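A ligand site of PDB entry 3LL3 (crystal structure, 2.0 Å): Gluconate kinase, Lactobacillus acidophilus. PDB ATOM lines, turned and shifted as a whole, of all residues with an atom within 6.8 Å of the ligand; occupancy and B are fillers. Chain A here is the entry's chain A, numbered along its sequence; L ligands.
The guanidinium group of Arg 344 lies within hydrogen-bond range of an oxygen (O3) of the ligand.
The side-chain carboxylate of Asp 239 sits at hydrogen-bond distance from an oxygen (O5) of the ligand.
O2 of the ligand sits at hydrogen-bond distance from NE2 of His 81 (2.9 Å).
An oxygen (O5) of the ligand is in hydrogen-bond range of the backbone NH of Met 80, 3.0 Å away.
OD1 of Asn 297 is in hydrogen-bond range of NE of Arg 344.
N of Asp 239 lies within hydrogen-bond range of O of Ser 78.
N of Phe 281 is in hydrogen-bond range of O of Gly 293 (2.9 Å).
N of Leu 291 sits at hydrogen-bond distance from O of Tyr 283, 2.8 Å away.
CA of Gln 79 touches O5 of the ligand, at 3.5 Å.
Trp 99 touches the ligand.
Arg 266 touches the ligand.
Phe 281 touches the ligand (CE2 to O1, 3.4 Å).
Tyr 283 touches the ligand.
CB of Pro 295 touches O3 of the ligand, 3.7 Å away.
Hydrophobic or aromatic side chains that line the ligand: Met 80, His 81, Trp 99, Phe 281 and Pro 295.
Ten residues have an atom within 4 Å of the ligand: Gln 79, Met 80, His 81, Trp 99, Asp 239, Arg 266, Phe 281, Tyr 283, Pro 295 and Arg 344.
The nearest printed residue that does not touch the ligand is Met 131 (4.1 Å).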
ATOM      1  N   THR A  13       5.177  33.536  17.199  1.00  0.00           N
ATOM      2  CA  THR A  13       4.624  34.801  17.665  1.00  0.00           C
ATOM      3  C   THR A  13       5.396  35.887  16.925  1.00  0.00           C
ATOM      4  O   THR A  13       6.569  35.699  16.562  1.00  0.00           O
ATOM      5  CB  THR A  13       4.781  34.946  19.191  1.00  0.00           C
ATOM      6  OG1 THR A  13       6.103  34.540  19.576  1.00  0.00           O
ATOM      7  CG2 THR A  13       3.784  34.058  19.911  1.00  0.00           C
ATOM      8  N   SER A  78       4.720  25.251  14.637  1.00  0.00           N
ATOM      9  CA  SER A  78       3.884  26.301  15.201  1.00  0.00           C
ATOM     10  C   SER A  78       4.179  26.587  16.668  1.00  0.00           C
ATOM     11  O   SER A  78       4.488  25.672  17.435  1.00  0.00           O
ATOM     12  CB  SER A  78       2.405  25.927  15.022  1.00  0.00           C
ATOM     13  OG  SER A  78       1.560  26.846  15.678  1.00  0.00           O
ATOM     14  N   GLN A  79       4.061  27.858  17.060  1.00  0.00           N
ATOM     15  CA  GLN A  79       4.034  28.247  18.461  1.00  0.00           C
ATOM     16  C   GLN A  79       3.032  27.371  19.202  1.00  0.00           C
ATOM     17  O   GLN A  79       2.102  26.847  18.600  1.00  0.00           O
ATOM     18  CB  GLN A  79       3.589  29.709  18.580  1.00  0.00           C
ATOM     19  CG  GLN A  79       2.156  29.908  18.119  1.00  0.00           C
ATOM     20  CD  GLN A  79       1.769  31.376  18.016  1.00  0.00           C
ATOM     21  OE1 GLN A  79       1.949  32.014  16.980  1.00  0.00           O
ATOM     22  NE2 GLN A  79       1.186  31.904  19.085  1.00  0.00           N
ATOM     23  N   MET A  80       3.234  27.215  20.504  1.00  0.00           N
ATOM     24  CA  MET A  80       2.403  26.363  21.339  1.00  0.00           C
ATOM     25  C   MET A  80       1.500  27.175  22.258  1.00  0.00           C
ATOM     26  O   MET A  80       1.725  28.360  22.455  1.00  0.00           O
ATOM     27  CB  MET A  80       3.268  25.456  22.187  1.00  0.00           C
ATOM     28  CG  MET A  80       4.169  24.556  21.368  1.00  0.00           C
ATOM     29  SD  MET A  80       5.168  23.297  22.501  1.00  0.00           S
ATOM     30  CE  MET A  80       3.675  22.033  22.871  1.00  0.00           C
ATOM     31  N   HIS A  81       0.469  26.508  22.783  1.00  0.00           N
ATOM     32  CA  HIS A  81      -0.327  27.025  23.883  1.00  0.00           C
ATOM     33  C   HIS A  81      -1.318  28.126  23.460  1.00  0.00           C
ATOM     34  O   HIS A  81      -1.970  28.716  24.313  1.00  0.00           O
ATOM     35  CB  HIS A  81       0.571  27.554  25.021  1.00  0.00           C
ATOM     36  CG  HIS A  81       1.703  26.642  25.385  1.00  0.00           C
ATOM     37  ND1 HIS A  81       1.528  25.329  25.735  1.00  0.00           N
ATOM     38  CD2 HIS A  81       3.031  26.877  25.470  1.00  0.00           C
ATOM     39  CE1 HIS A  81       2.700  24.778  25.997  1.00  0.00           C
ATOM     40  NE2 HIS A  81       3.634  25.695  25.854  1.00  0.00           N
ATOM     41  N   TRP A  99       0.764  32.085  24.196  1.00  0.00           N
ATOM     42  CA  TRP A  99       1.319  31.512  25.410  1.00  0.00           C
ATOM     43  C   TRP A  99       1.668  32.621  26.410  1.00  0.00           C
ATOM     44  O   TRP A  99       1.593  32.396  27.602  1.00  0.00           O
ATOM     45  CB  TRP A  99       2.557  30.678  25.101  1.00  0.00           C
ATOM     46  CG  TRP A  99       3.704  31.513  24.678  1.00  0.00           C
ATOM     47  CD1 TRP A  99       4.022  31.920  23.412  1.00  0.00           C
ATOM     48  CD2 TRP A  99       4.694  32.101  25.535  1.00  0.00           C
ATOM     49  NE1 TRP A  99       5.145  32.701  23.426  1.00  0.00           N
ATOM     50  CE2 TRP A  99       5.575  32.829  24.718  1.00  0.00           C
ATOM     51  CE3 TRP A  99       4.926  32.063  26.913  1.00  0.00           C
ATOM     52  CZ2 TRP A  99       6.669  33.531  25.234  1.00  0.00           C
ATOM     53  CZ3 TRP A  99       6.000  32.745  27.426  1.00  0.00           C
ATOM     54  CH2 TRP A  99       6.873  33.473  26.587  1.00  0.00           C
ATOM     55  N   MET A 126       1.621  19.222  31.957  1.00  0.00           N
ATOM     56  CA  MET A 126       1.606  20.676  31.860  1.00  0.00           C
ATOM     57  C   MET A 126       2.029  21.359  33.156  1.00  0.00           C
ATOM     58  O   MET A 126       1.373  21.227  34.188  1.00  0.00           O
ATOM     59  CB  MET A 126       0.220  21.174  31.433  1.00  0.00           C
ATOM     60  CG  MET A 126       0.085  22.693  31.452  1.00  0.00           C
ATOM     61  SD  MET A 126       1.366  23.518  30.183  1.00  0.00           S
ATOM     62  CE  MET A 126       1.288  25.368  30.805  1.00  0.00           C
ATOM     63  N   MET A 131       0.175  29.957  30.800  1.00  0.00           N
ATOM     64  CA  MET A 131       0.343  29.841  29.350  1.00  0.00           C
ATOM     65  C   MET A 131      -0.590  28.784  28.724  1.00  0.00           C
ATOM     66  O   MET A 131      -0.951  28.885  27.552  1.00  0.00           O
ATOM     67  CB  MET A 131       1.795  29.488  29.025  1.00  0.00           C
ATOM     68  CG  MET A 131       2.218  28.101  29.502  1.00  0.00           C
ATOM     69  SD  MET A 131       4.188  27.808  29.353  1.00  0.00           S
ATOM     70  CE  MET A 131       4.357  26.013  30.091  1.00  0.00           C
ATOM     71  N   ASP A 239       6.644  23.767  17.687  1.00  0.00           N
ATOM     72  CA  ASP A 239       8.004  24.278  17.515  1.00  0.00           C
ATOM     73  C   ASP A 239       8.970  23.592  18.476  1.00  0.00           C
ATOM     74  O   ASP A 239      10.113  23.303  18.133  1.00  0.00           O
ATOM     75  CB  ASP A 239       8.016  25.803  17.704  1.00  0.00           C
ATOM     76  CG  ASP A 239       7.404  26.246  19.036  1.00  0.00           C
ATOM     77  OD1 ASP A 239       7.009  25.383  19.849  1.00  0.00           O
ATOM     78  OD2 ASP A 239       7.302  27.475  19.273  1.00  0.00           O
ATOM     79  N   GLY A 240       8.505  23.308  19.693  1.00  0.00           N
ATOM     80  CA  GLY A 240       9.312  22.618  20.689  1.00  0.00           C
ATOM     81  C   GLY A 240       9.780  21.234  20.258  1.00  0.00           C
ATOM     82  O   GLY A 240      10.960  20.898  20.376  1.00  0.00           O
ATOM     83  N   SER A 262      15.225  34.123  24.335  1.00  0.00           N
ATOM     84  CA  SER A 262      14.932  33.241  25.448  1.00  0.00           C
ATOM     85  C   SER A 262      15.587  31.898  25.163  1.00  0.00           C
ATOM     86  O   SER A 262      16.150  31.716  24.086  1.00  0.00           O
ATOM     87  CB  SER A 262      13.418  33.100  25.638  1.00  0.00           C
ATOM     88  OG  SER A 262      12.801  32.519  24.477  1.00  0.00           O
ATOM     89  N   GLY A 263      15.535  30.955  26.082  1.00  0.00           N
ATOM     90  CA  GLY A 263      16.122  29.649  25.837  1.00  0.00           C
ATOM     91  C   GLY A 263      15.206  28.477  26.113  1.00  0.00           C
ATOM     92  O   GLY A 263      14.083  28.642  26.601  1.00  0.00           O
ATOM     93  N   ALA A 264      15.690  27.272  25.812  1.00  0.00           N
ATOM     94  CA  ALA A 264      14.987  26.042  26.143  1.00  0.00           C
ATOM     95  C   ALA A 264      15.974  24.879  26.200  1.00  0.00           C
ATOM     96  O   ALA A 264      16.896  24.805  25.387  1.00  0.00           O
ATOM     97  CB  ALA A 264      13.886  25.769  25.130  1.00  0.00           C
ATOM     98  N   ARG A 266      15.687  20.643  26.172  1.00  0.00           N
ATOM     99  CA  ARG A 266      14.732  19.570  25.892  1.00  0.00           C
ATOM    100  C   ARG A 266      15.390  18.239  25.563  1.00  0.00           C
ATOM    101  O   ARG A 266      16.528  18.176  25.076  1.00  0.00           O
ATOM    102  CB  ARG A 266      13.886  19.927  24.692  1.00  0.00           C
ATOM    103  CG  ARG A 266      13.192  21.238  24.767  1.00  0.00           C
ATOM    104  CD  ARG A 266      12.513  21.487  23.443  1.00  0.00           C
ATOM    105  NE  ARG A 266      11.880  22.797  23.391  1.00  0.00           N
ATOM    106  CZ  ARG A 266      12.321  23.821  22.658  1.00  0.00           C
ATOM    107  NH1 ARG A 266      13.416  23.687  21.905  1.00  0.00           N
ATOM    108  NH2 ARG A 266      11.643  24.970  22.673  1.00  0.00           N
ATOM    109  N   PHE A 281       8.215  20.300  31.731  1.00  0.00           N
ATOM    110  CA  PHE A 281       7.014  19.797  31.105  1.00  0.00           C
ATOM    111  C   PHE A 281       7.261  18.412  30.541  1.00  0.00           C
ATOM    112  O   PHE A 281       8.422  18.022  30.318  1.00  0.00           O
ATOM    113  CB  PHE A 281       6.493  20.756  30.016  1.00  0.00           C
ATOM    114  CG  PHE A 281       7.463  20.958  28.841  1.00  0.00           C
ATOM    115  CD1 PHE A 281       7.769  19.905  27.977  1.00  0.00           C
ATOM    116  CD2 PHE A 281       8.005  22.202  28.578  1.00  0.00           C
ATOM    117  CE1 PHE A 281       8.607  20.092  26.879  1.00  0.00           C
ATOM    118  CE2 PHE A 281       8.866  22.396  27.486  1.00  0.00           C
ATOM    119  CZ  PHE A 281       9.158  21.344  26.642  1.00  0.00           C
ATOM    120  N   TYR A 283       5.529  16.611  27.241  1.00  0.00           N
ATOM    121  CA  TYR A 283       4.597  16.746  26.118  1.00  0.00           C
ATOM    122  C   TYR A 283       4.745  15.547  25.196  1.00  0.00           C
ATOM    123  O   TYR A 283       5.758  15.417  24.483  1.00  0.00           O
ATOM    124  CB  TYR A 283       4.861  18.013  25.282  1.00  0.00           C
ATOM    125  CG  TYR A 283       4.785  19.344  26.021  1.00  0.00           C
ATOM    126  CD1 TYR A 283       3.987  19.492  27.150  1.00  0.00           C
ATOM    127  CD2 TYR A 283       5.483  20.452  25.561  1.00  0.00           C
ATOM    128  CE1 TYR A 283       3.900  20.709  27.806  1.00  0.00           C
ATOM    129  CE2 TYR A 283       5.419  21.676  26.223  1.00  0.00           C
ATOM    130  CZ  TYR A 283       4.615  21.792  27.350  1.00  0.00           C
ATOM    131  OH  TYR A 283       4.519  22.998  28.005  1.00  0.00           O
ATOM    132  N   LEU A 291       8.338  14.503  24.942  1.00  0.00           N
ATOM    133  CA  LEU A 291       9.239  15.649  24.965  1.00  0.00           C
ATOM    134  C   LEU A 291       9.292  16.245  26.359  1.00  0.00           C
ATOM    135  O   LEU A 291       8.283  16.755  26.875  1.00  0.00           O
ATOM    136  CB  LEU A 291       8.810  16.700  23.934  1.00  0.00           C
ATOM    137  CG  LEU A 291       9.739  17.920  23.801  1.00  0.00           C
ATOM    138  CD1 LEU A 291      10.998  17.555  23.004  1.00  0.00           C
ATOM    139  CD2 LEU A 291       8.976  19.049  23.103  1.00  0.00           C
ATOM    140  N   GLY A 293      11.085  19.083  28.838  1.00  0.00           N
ATOM    141  CA  GLY A 293      11.893  20.273  28.744  1.00  0.00           C
ATOM    142  C   GLY A 293      11.576  21.391  29.698  1.00  0.00           C
ATOM    143  O   GLY A 293      10.594  21.332  30.465  1.00  0.00           O
ATOM    144  N   GLY A 294      12.429  22.399  29.643  1.00  0.00           N
ATOM    145  CA  GLY A 294      12.266  23.626  30.389  1.00  0.00           C
ATOM    146  C   GLY A 294      12.401  24.830  29.466  1.00  0.00           C
ATOM    147  O   GLY A 294      13.445  25.034  28.850  1.00  0.00           O
ATOM    148  N   PRO A 295      11.324  25.604  29.333  1.00  0.00           N
ATOM    149  CA  PRO A 295      11.441  26.882  28.633  1.00  0.00           C
ATOM    150  C   PRO A 295      12.036  27.902  29.616  1.00  0.00           C
ATOM    151  O   PRO A 295      11.614  27.955  30.754  1.00  0.00           O
ATOM    152  CB  PRO A 295       9.991  27.250  28.323  1.00  0.00           C
ATOM    153  CG  PRO A 295       9.132  26.376  29.221  1.00  0.00           C
ATOM    154  CD  PRO A 295      10.005  25.435  29.984  1.00  0.00           C
ATOM    155  N   VAL A 296      13.035  28.652  29.190  1.00  0.00           N
ATOM    156  CA  VAL A 296      13.754  29.550  30.098  1.00  0.00           C
ATOM    157  C   VAL A 296      13.701  30.966  29.528  1.00  0.00           C
ATOM    158  O   VAL A 296      14.172  31.205  28.394  1.00  0.00           O
ATOM    159  CB  VAL A 296      15.222  29.100  30.243  1.00  0.00           C
ATOM    160  CG1 VAL A 296      15.984  30.055  31.150  1.00  0.00           C
ATOM    161  CG2 VAL A 296      15.293  27.688  30.806  1.00  0.00           C
ATOM    162  N   ASN A 297      13.125  31.896  30.275  1.00  0.00           N
ATOM    163  CA  ASN A 297      12.948  33.262  29.784  1.00  0.00           C
ATOM    164  C   ASN A 297      14.279  33.990  29.549  1.00  0.00           C
ATOM    165  O   ASN A 297      14.460  34.689  28.546  1.00  0.00           O
ATOM    166  CB  ASN A 297      12.108  34.116  30.747  1.00  0.00           C
ATOM    167  CG  ASN A 297      10.716  33.536  31.006  1.00  0.00           C
ATOM    168  OD1 ASN A 297      10.188  32.768  30.205  1.00  0.00           O
ATOM    169  ND2 ASN A 297      10.109  33.944  32.130  1.00  0.00           N
ATOM    170  N   ARG A 344      10.388  30.936  34.129  1.00  0.00           N
ATOM    171  CA  ARG A 344       9.696  29.661  34.060  1.00  0.00           C
ATOM    172  C   ARG A 344      10.676  28.591  34.554  1.00  0.00           C
ATOM    173  O   ARG A 344      11.088  28.648  35.704  1.00  0.00           O
ATOM    174  CB  ARG A 344       9.104  29.417  32.655  1.00  0.00           C
ATOM    175  CG  ARG A 344       7.849  30.288  32.436  1.00  0.00           C
ATOM    176  CD  ARG A 344       7.284  30.252  31.023  1.00  0.00           C
ATOM    177  NE  ARG A 344       8.198  30.888  30.079  1.00  0.00           N
ATOM    178  CZ  ARG A 344       8.257  30.593  28.776  1.00  0.00           C
ATOM    179  NH1 ARG A 344       7.451  29.674  28.267  1.00  0.00           N
ATOM    180  NH2 ARG A 344       9.138  31.218  28.001  1.00  0.00           N
ATOM    181  N   TRP A 348      10.189  28.515  38.131  1.00  0.00           N
ATOM    182  CA  TRP A 348       8.742  28.723  37.990  1.00  0.00           C
ATOM    183  C   TRP A 348       8.228  29.744  39.007  1.00  0.00           C
ATOM    184  O   TRP A 348       7.359  29.449  39.824  1.00  0.00           O
ATOM    185  CB  TRP A 348       7.976  27.390  38.072  1.00  0.00           C
ATOM    186  CG  TRP A 348       8.325  26.471  36.917  1.00  0.00           C
ATOM    187  CD1 TRP A 348       9.212  25.415  36.931  1.00  0.00           C
ATOM    188  CD2 TRP A 348       7.811  26.542  35.578  1.00  0.00           C
ATOM    189  NE1 TRP A 348       9.283  24.832  35.674  1.00  0.00           N
ATOM    190  CE2 TRP A 348       8.429  25.496  34.833  1.00  0.00           C
ATOM    191  CE3 TRP A 348       6.902  27.375  34.931  1.00  0.00           C
ATOM    192  CZ2 TRP A 348       8.172  25.284  33.476  1.00  0.00           C
ATOM    193  CZ3 TRP A 348       6.630  27.156  33.589  1.00  0.00           C
ATOM    194  CH2 TRP A 348       7.270  26.115  32.874  1.00  0.00           C
HETATM  195  C1  LIG L   1       7.528  25.245  24.494  1.00  0.00           C
HETATM  196  C2  LIG L   1       6.807  26.212  25.452  1.00  0.00           C
HETATM  197  C3  LIG L   1       6.640  27.707  25.078  1.00  0.00           C
HETATM  198  C4  LIG L   1       6.923  28.068  23.605  1.00  0.00           C
HETATM  199  C5  LIG L   1       5.841  27.569  22.630  1.00  0.00           C
HETATM  200  O1  LIG L   1       8.728  24.790  25.081  1.00  0.00           O
HETATM  201  O2  LIG L   1       6.428  25.801  26.522  1.00  0.00           O
HETATM  202  O3  LIG L   1       7.530  28.486  25.841  1.00  0.00           O
HETATM  203  O4  LIG L   1       6.994  29.470  23.514  1.00  0.00           O
HETATM  204  O5  LIG L   1       5.826  28.329  21.443  1.00  0.00           O
